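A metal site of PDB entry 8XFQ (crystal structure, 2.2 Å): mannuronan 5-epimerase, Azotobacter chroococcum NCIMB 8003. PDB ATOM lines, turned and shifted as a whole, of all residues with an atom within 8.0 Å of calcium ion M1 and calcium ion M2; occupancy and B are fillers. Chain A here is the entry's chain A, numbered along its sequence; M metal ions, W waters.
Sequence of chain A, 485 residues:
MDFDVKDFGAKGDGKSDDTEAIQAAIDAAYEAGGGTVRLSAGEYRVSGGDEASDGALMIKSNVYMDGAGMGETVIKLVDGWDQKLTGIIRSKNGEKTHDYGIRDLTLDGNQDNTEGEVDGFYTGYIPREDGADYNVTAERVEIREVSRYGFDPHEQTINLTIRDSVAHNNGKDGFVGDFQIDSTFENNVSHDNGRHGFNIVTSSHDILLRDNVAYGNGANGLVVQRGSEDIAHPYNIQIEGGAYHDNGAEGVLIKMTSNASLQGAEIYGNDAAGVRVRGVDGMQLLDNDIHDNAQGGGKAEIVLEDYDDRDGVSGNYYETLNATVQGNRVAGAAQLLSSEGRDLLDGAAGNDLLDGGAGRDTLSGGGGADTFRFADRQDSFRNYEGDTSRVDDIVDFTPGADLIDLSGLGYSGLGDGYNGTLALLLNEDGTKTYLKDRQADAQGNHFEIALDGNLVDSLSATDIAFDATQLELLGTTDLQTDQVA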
ATOM      1  N   VAL A 330     -25.199  36.123  28.362  1.00  0.00           N
ATOM      2  CA  VAL A 330     -26.461  35.462  28.698  1.00  0.00           C
ATOM      3  C   VAL A 330     -26.233  34.604  29.936  1.00  0.00           C
ATOM      4  O   VAL A 330     -25.558  33.573  29.860  1.00  0.00           O
ATOM      5  CB  VAL A 330     -26.995  34.610  27.533  1.00  0.00           C
ATOM      6  CG1 VAL A 330     -28.453  34.263  27.770  1.00  0.00           C
ATOM      7  CG2 VAL A 330     -26.842  35.344  26.200  1.00  0.00           C
ATOM      8  N   GLY A 332     -27.836  32.309  31.453  1.00  0.00           N
ATOM      9  CA  GLY A 332     -28.852  31.282  31.383  1.00  0.00           C
ATOM     10  C   GLY A 332     -28.849  30.608  30.037  1.00  0.00           C
ATOM     11  O   GLY A 332     -28.018  30.901  29.164  1.00  0.00           O
ATOM     12  N   ALA A 333     -29.809  29.701  29.860  1.00  0.00           N
ATOM     13  CA  ALA A 333     -29.851  28.861  28.684  1.00  0.00           C
ATOM     14  C   ALA A 333     -30.385  29.626  27.477  1.00  0.00           C
ATOM     15  O   ALA A 333     -31.340  30.409  27.579  1.00  0.00           O
ATOM     16  CB  ALA A 333     -30.722  27.631  28.942  1.00  0.00           C
ATOM     17  N   ALA A 334     -29.767  29.394  26.329  1.00  0.00           N
ATOM     18  CA  ALA A 334     -30.219  29.946  25.058  1.00  0.00           C
ATOM     19  C   ALA A 334     -30.665  28.807  24.158  1.00  0.00           C
ATOM     20  O   ALA A 334     -29.908  27.851  23.947  1.00  0.00           O
ATOM     21  CB  ALA A 334     -29.107  30.758  24.385  1.00  0.00           C
ATOM     22  N   ASP A 346     -24.053  31.563  18.284  1.00  0.00           N
ATOM     23  CA  ASP A 346     -23.132  31.447  19.408  1.00  0.00           C
ATOM     24  C   ASP A 346     -23.917  31.459  20.711  1.00  0.00           C
ATOM     25  O   ASP A 346     -24.706  32.376  20.958  1.00  0.00           O
ATOM     26  CB  ASP A 346     -22.113  32.594  19.427  1.00  0.00           C
ATOM     27  CG  ASP A 346     -21.347  32.724  18.125  1.00  0.00           C
ATOM     28  OD1 ASP A 346     -21.204  31.710  17.399  1.00  0.00           O
ATOM     29  OD2 ASP A 346     -20.845  33.838  17.848  1.00  0.00           O
ATOM     30  N   GLY A 347     -23.697  30.444  21.532  1.00  0.00           N
ATOM     31  CA  GLY A 347     -24.202  30.433  22.883  1.00  0.00           C
ATOM     32  C   GLY A 347     -23.324  31.271  23.805  1.00  0.00           C
ATOM     33  O   GLY A 347     -22.380  31.934  23.389  1.00  0.00           O
ATOM     34  N   ALA A 348     -23.662  31.212  25.083  1.00  0.00           N
ATOM     35  CA  ALA A 348     -22.998  32.026  26.104  1.00  0.00           C
ATOM     36  C   ALA A 348     -22.828  31.147  27.350  1.00  0.00           C
ATOM     37  O   ALA A 348     -22.835  29.917  27.268  1.00  0.00           O
ATOM     38  CB  ALA A 348     -23.778  33.322  26.361  1.00  0.00           C
ATOM     39  N   ALA A 349     -22.639  31.792  28.504  1.00  0.00           N
ATOM     40  CA  ALA A 349     -22.309  31.091  29.743  1.00  0.00           C
ATOM     41  C   ALA A 349     -23.280  29.958  30.098  1.00  0.00           C
ATOM     42  O   ALA A 349     -22.914  29.083  30.894  1.00  0.00           O
ATOM     43  CB  ALA A 349     -22.268  32.099  30.900  1.00  0.00           C
ATOM     44  N   GLY A 350     -24.497  29.945  29.548  1.00  0.00           N
ATOM     45  CA  GLY A 350     -25.470  28.952  29.945  1.00  0.00           C
ATOM     46  C   GLY A 350     -25.321  27.612  29.230  1.00  0.00           C
ATOM     47  O   GLY A 350     -24.500  27.433  28.336  1.00  0.00           O
ATOM     48  N   ASN A 351     -26.149  26.656  29.655  1.00  0.00           N
ATOM     49  CA  ASN A 351     -26.247  25.358  28.984  1.00  0.00           C
ATOM     50  C   ASN A 351     -27.227  25.503  27.819  1.00  0.00           C
ATOM     51  O   ASN A 351     -28.437  25.450  28.009  1.00  0.00           O
ATOM     52  CB  ASN A 351     -26.709  24.275  29.949  1.00  0.00           C
ATOM     53  CG  ASN A 351     -25.677  23.939  31.008  1.00  0.00           C
ATOM     54  OD1 ASN A 351     -24.533  24.393  30.938  1.00  0.00           O
ATOM     55  ND2 ASN A 351     -26.075  23.149  31.985  1.00  0.00           N
ATOM     56  N   ASP A 352     -26.695  25.680  26.619  1.00  0.00           N
ATOM     57  CA  ASP A 352     -27.488  26.074  25.462  1.00  0.00           C
ATOM     58  C   ASP A 352     -27.777  24.891  24.544  1.00  0.00           C
ATOM     59  O   ASP A 352     -27.064  23.885  24.546  1.00  0.00           O
ATOM     60  CB  ASP A 352     -26.778  27.186  24.694  1.00  0.00           C
ATOM     61  CG  ASP A 352     -26.316  28.319  25.589  1.00  0.00           C
ATOM     62  OD1 ASP A 352     -27.110  28.768  26.440  1.00  0.00           O
ATOM     63  OD2 ASP A 352     -25.164  28.768  25.442  1.00  0.00           O
ATOM     64  N   LEU A 353     -28.839  25.031  23.755  1.00  0.00           N
ATOM     65  CA  LEU A 353     -29.199  24.091  22.714  1.00  0.00           C
ATOM     66  C   LEU A 353     -29.056  24.781  21.367  1.00  0.00           C
ATOM     67  O   LEU A 353     -29.640  25.855  21.154  1.00  0.00           O
ATOM     68  CB  LEU A 353     -30.626  23.575  22.898  1.00  0.00           C
ATOM     69  CG  LEU A 353     -31.259  22.839  21.716  1.00  0.00           C
ATOM     70  CD1 LEU A 353     -30.531  21.530  21.453  1.00  0.00           C
ATOM     71  CD2 LEU A 353     -32.750  22.599  21.958  1.00  0.00           C
ATOM     72  N   LEU A 354     -28.293  24.169  20.456  1.00  0.00           N
ATOM     73  CA  LEU A 354     -27.992  24.789  19.174  1.00  0.00           C
ATOM     74  C   LEU A 354     -28.365  23.856  18.034  1.00  0.00           C
ATOM     75  O   LEU A 354     -28.010  22.669  18.053  1.00  0.00           O
ATOM     76  CB  LEU A 354     -26.509  25.174  19.085  1.00  0.00           C
ATOM     77  CG  LEU A 354     -26.135  26.273  20.080  1.00  0.00           C
ATOM     78  CD1 LEU A 354     -25.396  25.688  21.279  1.00  0.00           C
ATOM     79  CD2 LEU A 354     -25.300  27.349  19.397  1.00  0.00           C
ATOM     80  N   SER A 364     -21.372  27.674  17.991  1.00  0.00           N
ATOM     81  CA  SER A 364     -20.434  27.717  19.105  1.00  0.00           C
ATOM     82  C   SER A 364     -21.220  27.766  20.400  1.00  0.00           C
ATOM     83  O   SER A 364     -22.258  28.435  20.483  1.00  0.00           O
ATOM     84  CB  SER A 364     -19.494  28.933  18.999  1.00  0.00           C
ATOM     85  OG  SER A 364     -20.106  30.094  19.519  1.00  0.00           O
ATOM     86  N   GLY A 365     -20.727  27.056  21.406  1.00  0.00           N
ATOM     87  CA  GLY A 365     -21.430  26.970  22.665  1.00  0.00           C
ATOM     88  C   GLY A 365     -21.038  28.023  23.677  1.00  0.00           C
ATOM     89  O   GLY A 365     -21.882  28.483  24.452  1.00  0.00           O
ATOM     90  N   GLY A 366     -19.774  28.427  23.675  1.00  0.00           N
ATOM     91  CA  GLY A 366     -19.309  29.282  24.752  1.00  0.00           C
ATOM     92  C   GLY A 366     -19.169  28.493  26.036  1.00  0.00           C
ATOM     93  O   GLY A 366     -18.962  27.273  26.036  1.00  0.00           O
ATOM     94  N   GLY A 367     -19.301  29.190  27.163  1.00  0.00           N
ATOM     95  CA  GLY A 367     -19.191  28.543  28.458  1.00  0.00           C
ATOM     96  C   GLY A 367     -20.332  27.570  28.710  1.00  0.00           C
ATOM     97  O   GLY A 367     -21.346  27.533  28.003  1.00  0.00           O
ATOM     98  N   GLY A 368     -20.160  26.751  29.740  1.00  0.00           N
ATOM     99  CA  GLY A 368     -21.182  25.795  30.117  1.00  0.00           C
ATOM    100  C   GLY A 368     -21.183  24.540  29.251  1.00  0.00           C
ATOM    101  O   GLY A 368     -20.313  24.326  28.399  1.00  0.00           O
ATOM    102  N   ALA A 369     -22.179  23.692  29.496  1.00  0.00           N
ATOM    103  CA  ALA A 369     -22.335  22.422  28.784  1.00  0.00           C
ATOM    104  C   ALA A 369     -23.444  22.584  27.752  1.00  0.00           C
ATOM    105  O   ALA A 369     -24.627  22.716  28.117  1.00  0.00           O
ATOM    106  CB  ALA A 369     -22.641  21.281  29.750  1.00  0.00           C
ATOM    107  N   ASP A 370     -23.083  22.551  26.482  1.00  0.00           N
ATOM    108  CA  ASP A 370     -24.006  22.861  25.395  1.00  0.00           C
ATOM    109  C   ASP A 370     -24.257  21.625  24.525  1.00  0.00           C
ATOM    110  O   ASP A 370     -23.381  20.786  24.340  1.00  0.00           O
ATOM    111  CB  ASP A 370     -23.466  24.006  24.543  1.00  0.00           C
ATOM    112  CG  ASP A 370     -23.150  25.227  25.367  1.00  0.00           C
ATOM    113  OD1 ASP A 370     -24.099  25.773  25.989  1.00  0.00           O
ATOM    114  OD2 ASP A 370     -21.973  25.626  25.426  1.00  0.00           O
ATOM    115  N   THR A 371     -25.473  21.556  23.993  1.00  0.00           N
ATOM    116  CA  THR A 371     -25.894  20.457  23.125  1.00  0.00           C
ATOM    117  C   THR A 371     -26.037  20.988  21.698  1.00  0.00           C
ATOM    118  O   THR A 371     -26.801  21.929  21.452  1.00  0.00           O
ATOM    119  CB  THR A 371     -27.210  19.845  23.606  1.00  0.00           C
ATOM    120  OG1 THR A 371     -27.006  19.175  24.855  1.00  0.00           O
ATOM    121  CG2 THR A 371     -27.743  18.844  22.589  1.00  0.00           C
ATOM    122  N   PHE A 372     -25.304  20.382  20.765  1.00  0.00           N
ATOM    123  CA  PHE A 372     -25.403  20.698  19.347  1.00  0.00           C
ATOM    124  C   PHE A 372     -26.232  19.612  18.683  1.00  0.00           C
ATOM    125  O   PHE A 372     -25.767  18.486  18.501  1.00  0.00           O
ATOM    126  CB  PHE A 372     -24.022  20.813  18.715  1.00  0.00           C
ATOM    127  CG  PHE A 372     -23.117  21.801  19.403  1.00  0.00           C
ATOM    128  CD1 PHE A 372     -22.324  21.412  20.465  1.00  0.00           C
ATOM    129  CD2 PHE A 372     -23.082  23.126  18.991  1.00  0.00           C
ATOM    130  CE1 PHE A 372     -21.499  22.313  21.110  1.00  0.00           C
ATOM    131  CE2 PHE A 372     -22.254  24.041  19.629  1.00  0.00           C
ATOM    132  CZ  PHE A 372     -21.462  23.634  20.689  1.00  0.00           C
ATOM    133  N   ASP A 396     -16.138  25.449  19.053  1.00  0.00           N
ATOM    134  CA  ASP A 396     -15.498  25.277  20.357  1.00  0.00           C
ATOM    135  C   ASP A 396     -16.028  24.043  21.072  1.00  0.00           C
ATOM    136  O   ASP A 396     -16.278  24.078  22.276  1.00  0.00           O
ATOM    137  CB  ASP A 396     -15.724  26.514  21.222  1.00  0.00           C
ATOM    138  CG  ASP A 396     -17.196  26.775  21.517  1.00  0.00           C
ATOM    139  OD1 ASP A 396     -18.066  26.148  20.868  1.00  0.00           O
ATOM    140  OD2 ASP A 396     -17.491  27.602  22.409  1.00  0.00           O
ATOM    141  N   PHE A 397     -16.187  22.926  20.360  1.00  0.00           N
ATOM    142  CA  PHE A 397     -16.699  21.733  21.035  1.00  0.00           C
ATOM    143  C   PHE A 397     -15.724  21.285  22.115  1.00  0.00           C
ATOM    144  O   PHE A 397     -14.520  21.154  21.870  1.00  0.00           O
ATOM    145  CB  PHE A 397     -16.951  20.595  20.044  1.00  0.00           C
ATOM    146  CG  PHE A 397     -17.653  19.430  20.669  1.00  0.00           C
ATOM    147  CD1 PHE A 397     -19.037  19.439  20.817  1.00  0.00           C
ATOM    148  CD2 PHE A 397     -16.953  18.343  21.150  1.00  0.00           C
ATOM    149  CE1 PHE A 397     -19.700  18.378  21.409  1.00  0.00           C
ATOM    150  CE2 PHE A 397     -17.608  17.270  21.738  1.00  0.00           C
ATOM    151  CZ  PHE A 397     -18.984  17.299  21.866  1.00  0.00           C
ATOM    152  N   THR A 398     -16.254  21.050  23.311  1.00  0.00           N
ATOM    153  CA  THR A 398     -15.446  20.763  24.485  1.00  0.00           C
ATOM    154  C   THR A 398     -15.733  19.335  24.923  1.00  0.00           C
ATOM    155  O   THR A 398     -16.795  19.067  25.518  1.00  0.00           O
ATOM    156  CB  THR A 398     -15.755  21.757  25.609  1.00  0.00           C
ATOM    157  OG1 THR A 398     -15.130  23.012  25.311  1.00  0.00           O
ATOM    158  CG2 THR A 398     -15.193  21.264  26.934  1.00  0.00           C
ATOM    159  N   ALA A 401     -17.722  17.933  28.258  1.00  0.00           N
ATOM    160  CA  ALA A 401     -18.728  18.898  28.691  1.00  0.00           C
ATOM    161  C   ALA A 401     -19.878  19.037  27.707  1.00  0.00           C
ATOM    162  O   ALA A 401     -21.036  18.911  28.099  1.00  0.00           O
ATOM    163  CB  ALA A 401     -18.072  20.270  28.930  1.00  0.00           C
ATOM    164  N   ASP A 402     -19.582  19.292  26.431  1.00  0.00           N
ATOM    165  CA  ASP A 402     -20.624  19.484  25.434  1.00  0.00           C
ATOM    166  C   ASP A 402     -21.135  18.128  24.934  1.00  0.00           C
ATOM    167  O   ASP A 402     -20.635  17.058  25.298  1.00  0.00           O
ATOM    168  CB  ASP A 402     -20.110  20.330  24.283  1.00  0.00           C
ATOM    169  CG  ASP A 402     -19.673  21.719  24.724  1.00  0.00           C
ATOM    170  OD1 ASP A 402     -20.200  22.218  25.742  1.00  0.00           O
ATOM    171  OD2 ASP A 402     -18.813  22.310  24.048  1.00  0.00           O
ATOM    172  N   LEU A 403     -22.167  18.176  24.085  1.00  0.00           N
ATOM    173  CA  LEU A 403     -22.770  16.977  23.537  1.00  0.00           C
ATOM    174  C   LEU A 403     -23.203  17.215  22.100  1.00  0.00           C
ATOM    175  O   LEU A 403     -23.781  18.265  21.785  1.00  0.00           O
ATOM    176  CB  LEU A 403     -23.971  16.513  24.374  1.00  0.00           C
ATOM    177  CG  LEU A 403     -24.708  15.268  23.875  1.00  0.00           C
ATOM    178  CD1 LEU A 403     -23.862  14.025  24.069  1.00  0.00           C
ATOM    179  CD2 LEU A 403     -26.068  15.128  24.571  1.00  0.00           C
ATOM    180  N   THR A 476     -27.415  17.869  28.058  1.00  0.00           N
ATOM    181  CA  THR A 476     -26.882  18.937  28.889  1.00  0.00           C
ATOM    182  C   THR A 476     -27.906  20.025  29.195  1.00  0.00           C
ATOM    183  O   THR A 476     -27.599  20.953  29.951  1.00  0.00           O
ATOM    184  CB  THR A 476     -25.659  19.576  28.220  1.00  0.00           C
ATOM    185  OG1 THR A 476     -26.094  20.471  27.200  1.00  0.00           O
ATOM    186  CG2 THR A 476     -24.765  18.501  27.620  1.00  0.00           C
HETATM  187 CA    CA M   1     -23.074  27.819  26.381  1.00  0.00          CA
HETATM  188 CA    CA M   2     -19.615  24.786  26.131  1.00  0.00          CA
HETATM  189  O   HOH W   1     -19.076  24.758  23.386  1.00  0.00           O
HETATM  190  O   HOH W   2     -17.006  24.500  26.815  1.00  0.00           O
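O of Asp 370 sits at hydrogen-bond distance from N of Leu 403, 2.9 Å away. OD1 of Asp 396 is in hydrogen-bond range of N of Gly 365, at 2.9 Å. The side-chain carboxylate (OD1) of Asp 352 is in hydrogen-bond range of the backbone NH (N) of Ala 334 (2.7 Å). The backbone carbonyl oxygen (O) of Asp 352 is in hydrogen-bond range of the backbone NH (N) of Thr 371. The side-chain carboxylate (OD2) of Asp 396 sits at hydrogen-bond distance from the backbone NH (N) of Gly 366, at 2.7 Å. The side-chain carboxylate (OD2) of Asp 402 is in hydrogen-bond range of the backbone NH (N) of Thr 398 (2.9 Å).
Within 4 Å of calcium ion M2: Gly 366, Gly 367, Gly 368, Asp 370 and Asp 402.
Calcium ion M2 is bound by O of Gly 368 (2.4 Å), O of Gly 366 (2.6 Å), OD2 of Asp 370 (2.6 Å), OD1 of Asp 402 (2.7 Å), water W2 (2.7 Å) and water W1 (2.8 Å).
Calcium ion M1 is bound by O of Ala 348 (2.3 Å), OD1 of Asp 370 (2.3 Å), O of Gly 365 (2.4 Å), O of Gly 367 (2.4 Å), O of Gly 350 (2.5 Å), OD2 of Asp 352 (2.5 Å) and OD2 of Asp 370 (2.6 Å). Calcium ion M1 has seven donor atoms within binding distance.
Water W1 lies within hydrogen-bond range of OD2 of Asp 402 (2.5 Å), OD1 of Asp 396 (3.0 Å) and N of Gly 365 (3.5 Å).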
